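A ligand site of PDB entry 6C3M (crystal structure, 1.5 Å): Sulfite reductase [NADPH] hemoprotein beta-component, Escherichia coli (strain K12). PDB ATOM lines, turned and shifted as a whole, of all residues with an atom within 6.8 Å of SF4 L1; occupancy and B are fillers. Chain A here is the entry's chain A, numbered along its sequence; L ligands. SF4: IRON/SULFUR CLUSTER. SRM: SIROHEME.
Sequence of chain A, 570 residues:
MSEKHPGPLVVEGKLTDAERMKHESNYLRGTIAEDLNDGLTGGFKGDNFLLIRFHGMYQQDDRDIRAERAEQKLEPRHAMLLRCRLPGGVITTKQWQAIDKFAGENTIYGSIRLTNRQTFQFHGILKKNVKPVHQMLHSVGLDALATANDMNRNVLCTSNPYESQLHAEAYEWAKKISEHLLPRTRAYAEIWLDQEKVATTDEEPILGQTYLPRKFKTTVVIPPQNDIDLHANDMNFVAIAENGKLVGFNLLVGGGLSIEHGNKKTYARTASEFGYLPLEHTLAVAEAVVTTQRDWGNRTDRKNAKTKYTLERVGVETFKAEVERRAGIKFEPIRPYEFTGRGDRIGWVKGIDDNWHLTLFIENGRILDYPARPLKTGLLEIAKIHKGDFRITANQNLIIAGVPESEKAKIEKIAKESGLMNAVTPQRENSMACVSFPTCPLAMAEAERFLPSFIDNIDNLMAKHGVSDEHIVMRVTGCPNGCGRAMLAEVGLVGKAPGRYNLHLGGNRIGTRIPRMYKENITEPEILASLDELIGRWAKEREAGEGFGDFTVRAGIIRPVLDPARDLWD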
ATOM      1  N   ALA A 433      -9.442  -1.094  30.824  1.00  0.00           N
ATOM      2  CA  ALA A 433      -8.512  -1.056  29.695  1.00  0.00           C
ATOM      3  C   ALA A 433      -7.321  -0.177  30.015  1.00  0.00           C
ATOM      4  O   ALA A 433      -7.408   0.718  30.852  1.00  0.00           O
ATOM      5  CB  ALA A 433      -9.227  -0.538  28.437  1.00  0.00           C
ATOM      6  N   CYS A 434      -6.193  -0.404  29.328  1.00  0.00           N
ATOM      7  CA  CYS A 434      -5.031   0.480  29.450  1.00  0.00           C
ATOM      8  C   CYS A 434      -5.194   1.695  28.538  1.00  0.00           C
ATOM      9  O   CYS A 434      -6.078   1.750  27.714  1.00  0.00           O
ATOM     10  CB  CYS A 434      -3.761  -0.246  29.056  1.00  0.00           C
ATOM     11  SG  CYS A 434      -3.673  -0.540  27.268  1.00  0.00           S
ATOM     12  N   VAL A 435      -4.263   2.653  28.674  1.00  0.00           N
ATOM     13  CA  VAL A 435      -4.290   3.896  27.887  1.00  0.00           C
ATOM     14  C   VAL A 435      -4.223   3.617  26.383  1.00  0.00           C
ATOM     15  O   VAL A 435      -5.053   4.118  25.614  1.00  0.00           O
ATOM     16  CB  VAL A 435      -3.160   4.835  28.322  1.00  0.00           C
ATOM     17  CG1 VAL A 435      -3.055   6.024  27.373  1.00  0.00           C
ATOM     18  CG2 VAL A 435      -3.374   5.310  29.761  1.00  0.00           C
ATOM     19  N   SER A 436      -3.196   2.889  25.932  1.00  0.00           N
ATOM     20  CA  SER A 436      -2.992   2.584  24.506  1.00  0.00           C
ATOM     21  C   SER A 436      -2.960   3.883  23.675  1.00  0.00           C
ATOM     22  O   SER A 436      -2.452   4.916  24.130  1.00  0.00           O
ATOM     23  CB  SER A 436      -4.025   1.561  24.058  1.00  0.00           C
ATOM     24  OG  SER A 436      -3.786   1.184  22.710  1.00  0.00           O
ATOM     25  N   PHE A 437      -3.485   3.824  22.447  1.00  0.00           N
ATOM     26  CA  PHE A 437      -3.536   4.995  21.594  1.00  0.00           C
ATOM     27  C   PHE A 437      -4.447   6.056  22.237  1.00  0.00           C
ATOM     28  O   PHE A 437      -5.434   5.715  22.881  1.00  0.00           O
ATOM     29  CB  PHE A 437      -4.096   4.632  20.223  1.00  0.00           C
ATOM     30  CG  PHE A 437      -3.258   3.649  19.463  1.00  0.00           C
ATOM     31  CD1 PHE A 437      -2.029   4.001  18.924  1.00  0.00           C
ATOM     32  CD2 PHE A 437      -3.751   2.374  19.225  1.00  0.00           C
ATOM     33  CE1 PHE A 437      -1.307   3.084  18.187  1.00  0.00           C
ATOM     34  CE2 PHE A 437      -3.028   1.452  18.501  1.00  0.00           C
ATOM     35  CZ  PHE A 437      -1.812   1.805  17.978  1.00  0.00           C
ATOM     36  N   CYS A 440       0.252   6.153  23.823  1.00  0.00           N
ATOM     37  CA  CYS A 440       1.247   5.132  24.129  1.00  0.00           C
ATOM     38  C   CYS A 440       2.086   4.801  22.891  1.00  0.00           C
ATOM     39  O   CYS A 440       1.536   4.393  21.878  1.00  0.00           O
ATOM     40  CB  CYS A 440       0.605   3.854  24.642  1.00  0.00           C
ATOM     41  SG  CYS A 440       1.862   2.656  25.085  1.00  0.00           S
ATOM     42  N   PRO A 441       3.424   4.910  22.965  1.00  0.00           N
ATOM     43  CA  PRO A 441       4.239   4.579  21.796  1.00  0.00           C
ATOM     44  C   PRO A 441       4.309   3.105  21.484  1.00  0.00           C
ATOM     45  O   PRO A 441       4.813   2.734  20.409  1.00  0.00           O
ATOM     46  CB  PRO A 441       5.625   5.113  22.195  1.00  0.00           C
ATOM     47  CG  PRO A 441       5.659   4.968  23.646  1.00  0.00           C
ATOM     48  CD  PRO A 441       4.259   5.314  24.103  1.00  0.00           C
ATOM     49  N   LEU A 442       3.873   2.238  22.402  1.00  0.00           N
ATOM     50  CA  LEU A 442       4.029   0.802  22.254  1.00  0.00           C
ATOM     51  C   LEU A 442       2.739   0.113  21.818  1.00  0.00           C
ATOM     52  O   LEU A 442       2.735  -1.100  21.607  1.00  0.00           O
ATOM     53  CB  LEU A 442       4.549   0.204  23.568  1.00  0.00           C
ATOM     54  CG  LEU A 442       5.778   0.877  24.183  1.00  0.00           C
ATOM     55  CD1 LEU A 442       6.210   0.174  25.447  1.00  0.00           C
ATOM     56  CD2 LEU A 442       6.951   0.939  23.185  1.00  0.00           C
ATOM     57  N   ALA A 443       1.654   0.864  21.676  1.00  0.00           N
ATOM     58  CA  ALA A 443       0.340   0.275  21.432  1.00  0.00           C
ATOM     59  C   ALA A 443       0.266  -0.514  20.135  1.00  0.00           C
ATOM     60  O   ALA A 443       0.805  -0.107  19.093  1.00  0.00           O
ATOM     61  CB  ALA A 443      -0.732   1.371  21.404  1.00  0.00           C
ATOM     62  N   MET A 444      -0.408  -1.653  20.196  1.00  0.00           N
ATOM     63  CA  MET A 444      -0.726  -2.434  19.003  1.00  0.00           C
ATOM     64  C   MET A 444      -2.192  -2.330  18.591  1.00  0.00           C
ATOM     65  O   MET A 444      -2.493  -2.257  17.391  1.00  0.00           O
ATOM     66  CB  MET A 444      -0.361  -3.902  19.223  1.00  0.00           C
ATOM     67  CG  MET A 444       1.128  -4.101  19.504  1.00  0.00           C
ATOM     68  SD  MET A 444       1.509  -5.816  19.842  1.00  0.00           S
ATOM     69  CE  MET A 444       3.287  -5.781  20.096  1.00  0.00           C
ATOM     70  N   ALA A 445      -3.120  -2.296  19.558  1.00  0.00           N
ATOM     71  CA  ALA A 445      -4.545  -2.144  19.301  1.00  0.00           C
ATOM     72  C   ALA A 445      -5.100  -1.155  20.311  1.00  0.00           C
ATOM     73  O   ALA A 445      -4.537  -1.003  21.402  1.00  0.00           O
ATOM     74  CB  ALA A 445      -5.316  -3.473  19.418  1.00  0.00           C
ATOM     75  N   ALA A 447      -7.267   0.319  23.276  1.00  0.00           N
ATOM     76  CA  ALA A 447      -7.795  -0.262  24.507  1.00  0.00           C
ATOM     77  C   ALA A 447      -8.764   0.725  25.144  1.00  0.00           C
ATOM     78  O   ALA A 447      -9.978   0.540  25.028  1.00  0.00           O
ATOM     79  CB  ALA A 447      -6.656  -0.637  25.466  1.00  0.00           C
ATOM     80  N   VAL A 476      -9.067  -5.204  28.643  1.00  0.00           N
ATOM     81  CA  VAL A 476      -8.434  -5.042  27.340  1.00  0.00           C
ATOM     82  C   VAL A 476      -7.093  -4.364  27.514  1.00  0.00           C
ATOM     83  O   VAL A 476      -6.990  -3.296  28.139  1.00  0.00           O
ATOM     84  CB  VAL A 476      -9.319  -4.231  26.372  1.00  0.00           C
ATOM     85  CG1 VAL A 476      -8.691  -4.199  24.980  1.00  0.00           C
ATOM     86  CG2 VAL A 476     -10.724  -4.835  26.310  1.00  0.00           C
ATOM     87  N   THR A 477      -6.054  -4.968  26.969  1.00  0.00           N
ATOM     88  CA  THR A 477      -4.730  -4.371  27.057  1.00  0.00           C
ATOM     89  C   THR A 477      -4.210  -4.206  25.644  1.00  0.00           C
ATOM     90  O   THR A 477      -4.430  -5.078  24.801  1.00  0.00           O
ATOM     91  CB  THR A 477      -3.815  -5.231  27.999  1.00  0.00           C
ATOM     92  OG1 THR A 477      -2.749  -4.424  28.514  1.00  0.00           O
ATOM     93  CG2 THR A 477      -3.272  -6.519  27.324  1.00  0.00           C
ATOM     94  N   GLY A 478      -3.621  -3.033  25.369  1.00  0.00           N
ATOM     95  CA  GLY A 478      -3.282  -2.608  23.989  1.00  0.00           C
ATOM     96  C   GLY A 478      -2.108  -3.328  23.373  1.00  0.00           C
ATOM     97  O   GLY A 478      -1.926  -3.242  22.146  1.00  0.00           O
ATOM     98  N   CYS A 479      -1.307  -4.006  24.175  1.00  0.00           N
ATOM     99  CA  CYS A 479      -0.182  -4.800  23.724  1.00  0.00           C
ATOM    100  C   CYS A 479       0.177  -5.743  24.876  1.00  0.00           C
ATOM    101  O   CYS A 479      -0.388  -5.617  25.986  1.00  0.00           O
ATOM    102  CB  CYS A 479       1.004  -3.892  23.314  1.00  0.00           C
ATOM    103  SG  CYS A 479       2.078  -3.373  24.667  1.00  0.00           S
ATOM    104  N   PRO A 480       1.064  -6.709  24.663  1.00  0.00           N
ATOM    105  CA  PRO A 480       1.263  -7.754  25.673  1.00  0.00           C
ATOM    106  C   PRO A 480       2.092  -7.323  26.881  1.00  0.00           C
ATOM    107  O   PRO A 480       2.251  -8.122  27.806  1.00  0.00           O
ATOM    108  CB  PRO A 480       1.934  -8.881  24.878  1.00  0.00           C
ATOM    109  CG  PRO A 480       2.680  -8.167  23.795  1.00  0.00           C
ATOM    110  CD  PRO A 480       1.774  -7.023  23.403  1.00  0.00           C
ATOM    111  N   ASN A 481       2.570  -6.084  26.922  1.00  0.00           N
ATOM    112  CA  ASN A 481       3.132  -5.556  28.153  1.00  0.00           C
ATOM    113  C   ASN A 481       2.154  -5.713  29.299  1.00  0.00           C
ATOM    114  O   ASN A 481       2.564  -5.995  30.436  1.00  0.00           O
ATOM    115  CB  ASN A 481       3.510  -4.096  27.976  1.00  0.00           C
ATOM    116  CG  ASN A 481       4.802  -3.933  27.189  1.00  0.00           C
ATOM    117  OD1 ASN A 481       5.657  -4.839  27.163  1.00  0.00           O
ATOM    118  ND2 ASN A 481       4.963  -2.781  26.583  1.00  0.00           N
ATOM    119  N   GLY A 482       0.851  -5.574  29.021  1.00  0.00           N
ATOM    120  CA  GLY A 482      -0.148  -6.093  29.935  1.00  0.00           C
ATOM    121  C   GLY A 482      -0.666  -5.109  30.948  1.00  0.00           C
ATOM    122  O   GLY A 482      -1.243  -5.533  31.950  1.00  0.00           O
ATOM    123  N   CYS A 483      -0.469  -3.809  30.702  1.00  0.00           N
ATOM    124  CA  CYS A 483      -0.847  -2.767  31.655  1.00  0.00           C
ATOM    125  C   CYS A 483      -2.319  -2.817  32.030  1.00  0.00           C
ATOM    126  O   CYS A 483      -2.668  -2.424  33.146  1.00  0.00           O
ATOM    127  CB  CYS A 483      -0.523  -1.377  31.115  1.00  0.00           C
ATOM    128  SG  CYS A 483       1.146  -1.234  30.449  1.00  0.00           S
ATOM    129  N   GLY A 484      -3.192  -3.237  31.114  1.00  0.00           N
ATOM    130  CA  GLY A 484      -4.610  -3.312  31.454  1.00  0.00           C
ATOM    131  C   GLY A 484      -4.972  -4.494  32.336  1.00  0.00           C
ATOM    132  O   GLY A 484      -6.142  -4.639  32.700  1.00  0.00           O
HETATM  133 FE1  SF4 L   1      -1.380  -0.548  26.809  1.00  0.00          FE
HETATM  134 FE2  SF4 L   1       0.762   0.932  26.127  1.00  0.00          FE
HETATM  135 FE3  SF4 L   1       0.861  -1.770  25.829  1.00  0.00          FE
HETATM  136 FE4  SF4 L   1       0.756  -0.656  28.296  1.00  0.00          FE
HETATM  137  S1  SF4 L   1       2.364  -0.477  26.846  1.00  0.00           S
HETATM  138  S2  SF4 L   1      -0.398  -2.418  27.513  1.00  0.00           S
HETATM  139  S3  SF4 L   1      -0.495   1.147  27.905  1.00  0.00           S
HETATM  140  S4  SF4 L   1      -0.522  -0.310  24.811  1.00  0.00           S
HETATM  141 FE   SRM L   2       2.538   0.126  32.268  1.00  0.00          FE
HETATM  142  CHA SRM L   2       4.986   0.694  29.963  1.00  0.00           C
HETATM  143  CHB SRM L   2       0.775   2.764  31.037  1.00  0.00           C
HETATM  144  CHC SRM L   2       0.202  -0.316  34.666  1.00  0.00           C
HETATM  145  CHD SRM L   2       3.471  -3.140  32.493  1.00  0.00           C
HETATM  146  NA  SRM L   2       2.874   1.491  30.851  1.00  0.00           N
HETATM  147  C1A SRM L   2       3.976   1.627  30.048  1.00  0.00           C
HETATM  148  C2A SRM L   2       4.019   2.975  29.336  1.00  0.00           C
HETATM  149  CMA SRM L   2       4.830   4.010  30.105  1.00  0.00           C
HETATM  150  CDA SRM L   2       4.549   2.822  27.875  1.00  0.00           C
HETATM  151  CEA SRM L   2       6.024   3.160  27.671  1.00  0.00           C
HETATM  152  O3A SRM L   2       6.965   2.467  28.128  1.00  0.00           O
HETATM  153  O4A SRM L   2       6.340   4.160  26.971  1.00  0.00           O
HETATM  154  C3A SRM L   2       2.559   3.304  29.336  1.00  0.00           C
HETATM  155  CAA SRM L   2       2.187   4.727  29.011  1.00  0.00           C
HETATM  156  CBA SRM L   2       0.845   4.836  28.256  1.00  0.00           C
HETATM  157  CCA SRM L   2       0.376   6.267  28.195  1.00  0.00           C
HETATM  158  O1A SRM L   2       0.367   6.909  27.125  1.00  0.00           O
HETATM  159  O2A SRM L   2      -0.020   6.858  29.209  1.00  0.00           O
HETATM  160  C4A SRM L   2       1.986   2.464  30.439  1.00  0.00           C
HETATM  161  NB  SRM L   2       0.885   1.092  32.795  1.00  0.00           N
HETATM  162  C1B SRM L   2       0.278   2.155  32.204  1.00  0.00           C
HETATM  163  C2B SRM L   2      -0.979   2.551  32.928  1.00  0.00           C
HETATM  164  CMB SRM L   2      -1.192   4.078  32.894  1.00  0.00           C
HETATM  165  CDB SRM L   2      -2.188   1.819  32.329  1.00  0.00           C
HETATM  166  CEB SRM L   2      -3.545   2.338  32.751  1.00  0.00           C
HETATM  167  O3B SRM L   2      -4.437   2.549  31.905  1.00  0.00           O
HETATM  168  O4B SRM L   2      -3.794   2.581  33.958  1.00  0.00           O
HETATM  169  C3B SRM L   2      -0.625   2.052  34.303  1.00  0.00           C
HETATM  170  CAB SRM L   2       0.059   3.121  35.138  1.00  0.00           C
HETATM  171  CBB SRM L   2       0.395   2.497  36.503  1.00  0.00           C
HETATM  172  CCB SRM L   2       1.288   3.435  37.285  1.00  0.00           C
HETATM  173  O1B SRM L   2       0.774   4.449  37.814  1.00  0.00           O
HETATM  174  O2B SRM L   2       2.528   3.208  37.418  1.00  0.00           O
HETATM  175  C4B SRM L   2       0.174   0.856  33.930  1.00  0.00           C
HETATM  176  NC  SRM L   2       1.978  -1.426  33.385  1.00  0.00           N
HETATM  177  C1C SRM L   2       0.974  -1.421  34.295  1.00  0.00           C
HETATM  178  C2C SRM L   2       0.759  -2.769  34.878  1.00  0.00           C
HETATM  179  CDC SRM L   2      -0.371  -3.187  35.792  1.00  0.00           C
HETATM  180  CEC SRM L   2       0.003  -2.943  37.227  1.00  0.00           C
HETATM  181  O3C SRM L   2       1.171  -2.591  37.567  1.00  0.00           O
HETATM  182  O4C SRM L   2      -0.868  -3.104  38.116  1.00  0.00           O
HETATM  183  C3C SRM L   2       1.602  -3.672  34.106  1.00  0.00           C
HETATM  184  CAC SRM L   2       1.594  -5.193  34.137  1.00  0.00           C
HETATM  185  CBC SRM L   2       2.083  -5.737  35.502  1.00  0.00           C
HETATM  186  CCC SRM L   2       3.560  -5.985  35.326  1.00  0.00           C
HETATM  187  O1C SRM L   2       4.387  -5.043  35.397  1.00  0.00           O
HETATM  188  O2C SRM L   2       3.981  -7.134  35.080  1.00  0.00           O
HETATM  189  C4C SRM L   2       2.421  -2.718  33.285  1.00  0.00           C
HETATM  190  ND  SRM L   2       4.055  -0.944  31.529  1.00  0.00           N
HETATM  191  C1D SRM L   2       4.255  -2.292  31.699  1.00  0.00           C
HETATM  192  C2D SRM L   2       5.387  -2.809  30.884  1.00  0.00           C
HETATM  193  CAD SRM L   2       5.908  -4.207  30.757  1.00  0.00           C
HETATM  194  CBD SRM L   2       6.906  -4.394  31.895  1.00  0.00           C
HETATM  195  CCD SRM L   2       7.644  -5.704  31.803  1.00  0.00           C
HETATM  196  O1D SRM L   2       7.927  -6.327  32.828  1.00  0.00           O
HETATM  197  O2D SRM L   2       7.976  -6.177  30.714  1.00  0.00           O
HETATM  198  C3D SRM L   2       5.808  -1.651  30.109  1.00  0.00           C
HETATM  199  CDD SRM L   2       6.888  -1.600  29.055  1.00  0.00           C
HETATM  200  CED SRM L   2       8.260  -1.508  29.703  1.00  0.00           C
HETATM  201  O3D SRM L   2       8.476  -1.297  30.908  1.00  0.00           O
HETATM  202  O4D SRM L   2       9.264  -1.637  28.983  1.00  0.00           O
HETATM  203  C4D SRM L   2       4.935  -0.547  30.554  1.00  0.00           C
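The backbone NH of Cys 440 is in hydrogen-bond range of an oxygen (O1A) of SRM L2 (3.4 Å).
A sulfur (S2) of SF4 L1 lies close to the backbone NH (N) of Gly 482, at 3.7 Å.
FE of SRM L2 is bound by SG of Cys 483.
S1 of SF4 L1 sits close to ND2 of Asn 481 (3.5 Å).
SG of Cys 434 binds FE1 of SF4 L1 (2.3 Å).
The side-chain hydroxyl of Thr 477 lies close to a sulfur (S2) of SF4 L1, at 3.2 Å.
An iron atom (FE2) of SF4 L1 is bound by the side-chain sulfur (SG) of Cys 440, at 2.3 Å.
A sulfur (S3) of SF4 L1 lies close to the backbone NH (N) of Ser 436 (3.8 Å).
An iron atom (FE3) of SF4 L1 is bound by the side-chain sulfur (SG) of Cys 479.
An iron atom (FE4) of SF4 L1 is bound by the side-chain sulfur (SG) of Cys 483 (2.3 Å).
S2 of SF4 L1 sits close to N of Cys 483 (3.5 Å).
O3B of SRM L2 lies within hydrogen-bond range of N of Val 435 (3.2 Å).
N of Ser 436 sits close to SG of Cys 434.
The backbone carbonyl oxygen (O) of Gly 478 sits at hydrogen-bond distance from the backbone NH (N) of Ala 445, 3.0 Å away.
O of Gly 478 lies within hydrogen-bond range of N of Met 444, at 2.9 Å.
The side-chain hydroxyl of Thr 477 sits at hydrogen-bond distance from the backbone NH of Cys 483.
The side-chain sulfur (SG) of Cys 440 lies close to the backbone NH (N) of Leu 442 (3.4 Å).
The backbone carbonyl oxygen (O) of Val 476 sits at hydrogen-bond distance from the backbone NH (N) of Cys 434 (3.2 Å).
The side-chain sulfur of Cys 434 lies close to the backbone NH of Gly 478.
The side-chain hydroxyl (OG1) of Thr 477 sits at hydrogen-bond distance from the backbone NH (N) of Gly 484.
CB of Leu 442 touches S1 of SF4 L1, 3.998 Å away.
Ala 443 touches SF4 L1 (CA to S4, 3.5 Å).
Gly 478 touches SF4 L1 (N to FE1, 3.6 Å).
Hydrophobic or aromatic side chains within 4 Å of SF4 L1: Leu 442 and Ala 443.
11 residues have an atom within 4 Å of SF4 L1: Cys 434, Ser 436, Cys 440, Leu 442, Ala 443, Thr 477, Gly 478, Cys 479, Asn 481, Gly 482 and Cys 483.
The nearest printed residue that does not touch SF4 L1 is Val 435 (4.1 Å).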
